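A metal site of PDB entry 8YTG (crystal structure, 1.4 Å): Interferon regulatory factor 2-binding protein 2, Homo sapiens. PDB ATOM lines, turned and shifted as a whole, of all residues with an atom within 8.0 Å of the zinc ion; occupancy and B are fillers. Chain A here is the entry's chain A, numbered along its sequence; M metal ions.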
ATOM      1  N   CYS A  10      23.119  -4.413  17.747  1.00  0.00           N
ATOM      2  CA  CYS A  10      22.913  -4.494  19.182  1.00  0.00           C
ATOM      3  C   CYS A  10      23.136  -5.918  19.640  1.00  0.00           C
ATOM      4  O   CYS A  10      22.889  -6.872  18.905  1.00  0.00           O
ATOM      5  CB  CYS A  10      21.470  -4.106  19.515  1.00  0.00           C
ATOM      6  SG  CYS A  10      21.102  -2.348  19.318  1.00  0.00           S
ATOM      7  N   CYS A  11      23.572  -6.060  20.891  1.00  0.00           N
ATOM      8  CA  CYS A  11      23.734  -7.373  21.485  1.00  0.00           C
ATOM      9  C   CYS A  11      22.394  -8.095  21.575  1.00  0.00           C
ATOM     10  O   CYS A  11      21.402  -7.537  22.058  1.00  0.00           O
ATOM     11  CB  CYS A  11      24.294  -7.210  22.905  1.00  0.00           C
ATOM     12  SG  CYS A  11      24.500  -8.732  23.813  1.00  0.00           S
ATOM     13  N   THR A  12      22.383  -9.360  21.150  1.00  0.00           N
ATOM     14  CA  THR A  12      21.168 -10.168  21.168  1.00  0.00           C
ATOM     15  C   THR A  12      20.612 -10.345  22.583  1.00  0.00           C
ATOM     16  O   THR A  12      19.396 -10.426  22.765  1.00  0.00           O
ATOM     17  CB  THR A  12      21.484 -11.540  20.558  1.00  0.00           C
ATOM     18  OG1 THR A  12      21.827 -11.374  19.185  1.00  0.00           O
ATOM     19  CG2 THR A  12      20.310 -12.510  20.666  1.00  0.00           C
ATOM     20  N   LEU A  13      21.485 -10.398  23.586  1.00  0.00           N
ATOM     21  CA  LEU A  13      21.046 -10.686  24.948  1.00  0.00           C
ATOM     22  C   LEU A  13      20.679  -9.442  25.742  1.00  0.00           C
ATOM     23  O   LEU A  13      19.590  -9.384  26.331  1.00  0.00           O
ATOM     24  CB  LEU A  13      22.097 -11.537  25.673  1.00  0.00           C
ATOM     25  CG  LEU A  13      22.420 -12.883  24.998  1.00  0.00           C
ATOM     26  CD1 LEU A  13      23.569 -13.596  25.707  1.00  0.00           C
ATOM     27  CD2 LEU A  13      21.178 -13.770  24.960  1.00  0.00           C
ATOM     28  N   CYS A  14      21.569  -8.436  25.803  1.00  0.00           N
ATOM     29  CA  CYS A  14      21.319  -7.255  26.630  1.00  0.00           C
ATOM     30  C   CYS A  14      20.884  -6.013  25.842  1.00  0.00           C
ATOM     31  O   CYS A  14      20.540  -4.995  26.465  1.00  0.00           O
ATOM     32  CB  CYS A  14      22.557  -6.911  27.468  1.00  0.00           C
ATOM     33  SG  CYS A  14      23.886  -6.175  26.503  1.00  0.00           S
ATOM     34  N   HIS A  15      20.898  -6.078  24.511  1.00  0.00           N
ATOM     35  CA  HIS A  15      20.441  -5.038  23.587  1.00  0.00           C
ATOM     36  C   HIS A  15      21.362  -3.830  23.501  1.00  0.00           C
ATOM     37  O   HIS A  15      21.033  -2.860  22.825  1.00  0.00           O
ATOM     38  CB  HIS A  15      19.012  -4.609  23.883  1.00  0.00           C
ATOM     39  CG  HIS A  15      18.102  -5.772  24.143  1.00  0.00           C
ATOM     40  ND1 HIS A  15      17.720  -6.644  23.162  1.00  0.00           N
ATOM     41  CD2 HIS A  15      17.556  -6.222  25.297  1.00  0.00           C
ATOM     42  CE1 HIS A  15      16.942  -7.585  23.688  1.00  0.00           C
ATOM     43  NE2 HIS A  15      16.835  -7.349  24.981  1.00  0.00           N
ATOM     44  N   GLU A  16      22.533  -3.865  24.158  1.00  0.00           N
ATOM     45  CA  GLU A  16      23.461  -2.757  24.046  1.00  0.00           C
ATOM     46  C   GLU A  16      23.980  -2.585  22.629  1.00  0.00           C
ATOM     47  O   GLU A  16      24.296  -3.562  21.936  1.00  0.00           O
ATOM     48  CB  GLU A  16      24.637  -2.923  25.018  1.00  0.00           C
ATOM     49  CG  GLU A  16      25.476  -1.651  25.179  1.00  0.00           C
ATOM     50  CD  GLU A  16      24.841  -0.567  26.052  1.00  0.00           C
ATOM     51  OE1 GLU A  16      23.628  -0.651  26.371  1.00  0.00           O
ATOM     52  OE2 GLU A  16      25.576   0.381  26.417  1.00  0.00           O
ATOM     53  N   ARG A  17      24.066  -1.334  22.203  1.00  0.00           N
ATOM     54  CA  ARG A  17      24.652  -1.013  20.903  1.00  0.00           C
ATOM     55  C   ARG A  17      26.109  -1.456  20.859  1.00  0.00           C
ATOM     56  O   ARG A  17      26.879  -1.257  21.807  1.00  0.00           O
ATOM     57  CB  ARG A  17      24.539   0.489  20.697  1.00  0.00           C
ATOM     58  CG  ARG A  17      23.171   0.927  20.148  1.00  0.00           C
ATOM     59  CD  ARG A  17      23.064   2.435  20.169  1.00  0.00           C
ATOM     60  NE  ARG A  17      23.605   3.038  18.952  1.00  0.00           N
ATOM     61  CZ  ARG A  17      23.073   2.964  17.736  1.00  0.00           C
ATOM     62  NH1 ARG A  17      21.897   2.390  17.517  1.00  0.00           N
ATOM     63  NH2 ARG A  17      23.735   3.498  16.713  1.00  0.00           N
ATOM     64  N   LEU A  18      26.502  -2.060  19.738  1.00  0.00           N
ATOM     65  CA  LEU A  18      27.834  -2.653  19.622  1.00  0.00           C
ATOM     66  C   LEU A  18      28.876  -1.725  19.028  1.00  0.00           C
ATOM     67  O   LEU A  18      30.057  -2.101  19.004  1.00  0.00           O
ATOM     68  CB  LEU A  18      27.785  -3.951  18.818  1.00  0.00           C
ATOM     69  CG  LEU A  18      26.854  -5.012  19.400  1.00  0.00           C
ATOM     70  CD1 LEU A  18      26.626  -6.117  18.407  1.00  0.00           C
ATOM     71  CD2 LEU A  18      27.400  -5.544  20.742  1.00  0.00           C
ATOM     72  N   LYS A  33      24.556 -11.646  17.805  1.00  0.00           N
ATOM     73  CA  LYS A  33      25.744 -10.859  18.117  1.00  0.00           C
ATOM     74  C   LYS A  33      25.756 -10.597  19.617  1.00  0.00           C
ATOM     75  O   LYS A  33      24.718 -10.288  20.203  1.00  0.00           O
ATOM     76  CB  LYS A  33      25.795  -9.523  17.387  1.00  0.00           C
ATOM     77  CG  LYS A  33      25.735  -9.631  15.896  1.00  0.00           C
ATOM     78  CD  LYS A  33      25.321  -8.305  15.281  1.00  0.00           C
ATOM     79  CE  LYS A  33      24.599  -8.537  13.962  1.00  0.00           C
ATOM     80  NZ  LYS A  33      25.594  -8.650  12.854  1.00  0.00           N
ATOM     81  N   PHE A  34      26.922 -10.711  20.241  1.00  0.00           N
ATOM     82  CA  PHE A  34      27.003 -10.665  21.694  1.00  0.00           C
ATOM     83  C   PHE A  34      28.143  -9.778  22.149  1.00  0.00           C
ATOM     84  O   PHE A  34      29.282  -9.947  21.707  1.00  0.00           O
ATOM     85  CB  PHE A  34      27.159 -12.067  22.256  1.00  0.00           C
ATOM     86  CG  PHE A  34      26.180 -13.038  21.662  1.00  0.00           C
ATOM     87  CD1 PHE A  34      24.890 -13.123  22.164  1.00  0.00           C
ATOM     88  CD2 PHE A  34      26.536 -13.833  20.587  1.00  0.00           C
ATOM     89  CE1 PHE A  34      23.990 -13.995  21.606  1.00  0.00           C
ATOM     90  CE2 PHE A  34      25.646 -14.698  20.022  1.00  0.00           C
ATOM     91  CZ  PHE A  34      24.360 -14.791  20.534  1.00  0.00           C
ATOM     92  N   CYS A  35      27.840  -8.834  23.035  1.00  0.00           N
ATOM     93  CA  CYS A  35      28.899  -8.023  23.615  1.00  0.00           C
ATOM     94  C   CYS A  35      29.834  -8.884  24.453  1.00  0.00           C
ATOM     95  O   CYS A  35      29.520 -10.017  24.833  1.00  0.00           O
ATOM     96  CB  CYS A  35      28.313  -6.884  24.443  1.00  0.00           C
ATOM     97  SG  CYS A  35      27.494  -7.346  25.985  1.00  0.00           S
ATOM     98  N   PHE A  36      31.025  -8.340  24.737  1.00  0.00           N
ATOM     99  CA  PHE A  36      31.957  -9.072  25.595  1.00  0.00           C
ATOM    100  C   PHE A  36      31.433  -9.306  27.011  1.00  0.00           C
ATOM    101  O   PHE A  36      31.589 -10.433  27.504  1.00  0.00           O
ATOM    102  CB  PHE A  36      33.346  -8.432  25.592  1.00  0.00           C
ATOM    103  CG  PHE A  36      34.225  -8.847  24.438  1.00  0.00           C
ATOM    104  CD1 PHE A  36      33.708  -9.455  23.292  1.00  0.00           C
ATOM    105  CD2 PHE A  36      35.596  -8.625  24.497  1.00  0.00           C
ATOM    106  CE1 PHE A  36      34.551  -9.831  22.246  1.00  0.00           C
ATOM    107  CE2 PHE A  36      36.430  -8.999  23.456  1.00  0.00           C
ATOM    108  CZ  PHE A  36      35.906  -9.600  22.337  1.00  0.00           C
ATOM    109  N   PRO A  37      30.808  -8.336  27.696  1.00  0.00           N
ATOM    110  CA  PRO A  37      30.238  -8.676  29.013  1.00  0.00           C
ATOM    111  C   PRO A  37      29.271  -9.838  28.992  1.00  0.00           C
ATOM    112  O   PRO A  37      29.341 -10.706  29.871  1.00  0.00           O
ATOM    113  CB  PRO A  37      29.556  -7.359  29.444  1.00  0.00           C
ATOM    114  CG  PRO A  37      30.371  -6.298  28.776  1.00  0.00           C
ATOM    115  CD  PRO A  37      30.756  -6.895  27.440  1.00  0.00           C
ATOM    116  N   CYS A  38      28.363  -9.892  27.999  1.00  0.00           N
ATOM    117  CA  CYS A  38      27.444 -11.025  27.901  1.00  0.00           C
ATOM    118  C   CYS A  38      28.168 -12.309  27.511  1.00  0.00           C
ATOM    119  O   CYS A  38      27.846 -13.397  28.005  1.00  0.00           O
ATOM    120  CB  CYS A  38      26.345 -10.703  26.889  1.00  0.00           C
ATOM    121  SG  CYS A  38      25.100  -9.543  27.498  1.00  0.00           S
ATOM    122  N   SER A  39      29.162 -12.201  26.619  1.00  0.00           N
ATOM    123  CA  SER A  39      29.926 -13.382  26.252  1.00  0.00           C
ATOM    124  C   SER A  39      30.685 -13.947  27.442  1.00  0.00           C
ATOM    125  O   SER A  39      30.799 -15.170  27.600  1.00  0.00           O
ATOM    126  CB  SER A  39      30.873 -13.062  25.105  1.00  0.00           C
ATOM    127  OG  SER A  39      30.160 -12.676  23.935  1.00  0.00           O
HETATM  128 ZN    ZN M   1      25.239  -7.921  25.883  1.00  0.00          ZN
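Of the 16 residues printed, 4 come within 4 Å of the zinc ion.
N of Glu 16 lies close to SG of Cys 14, at 3.6 Å.
O of Cys 35 lies within hydrogen-bond range of OG of Ser 39 (2.9 Å).
The side-chain sulfur of Cys 11 lies close to the backbone NH of Leu 13 (3.5 Å).
The backbone carbonyl oxygen (O) of Glu 16 is in hydrogen-bond range of the backbone NH (N) of Cys 11, 2.8 Å away.
SG of Cys 38 is bound to the zinc ion.
The zinc ion is bound by SG of Cys 14 (2.3 Å).
SG of Cys 35 binds the zinc ion, at 2.3 Å.
The zinc ion is bound by SG of Cys 11 (2.3 Å).
The zinc ion has four donor atoms within binding distance.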
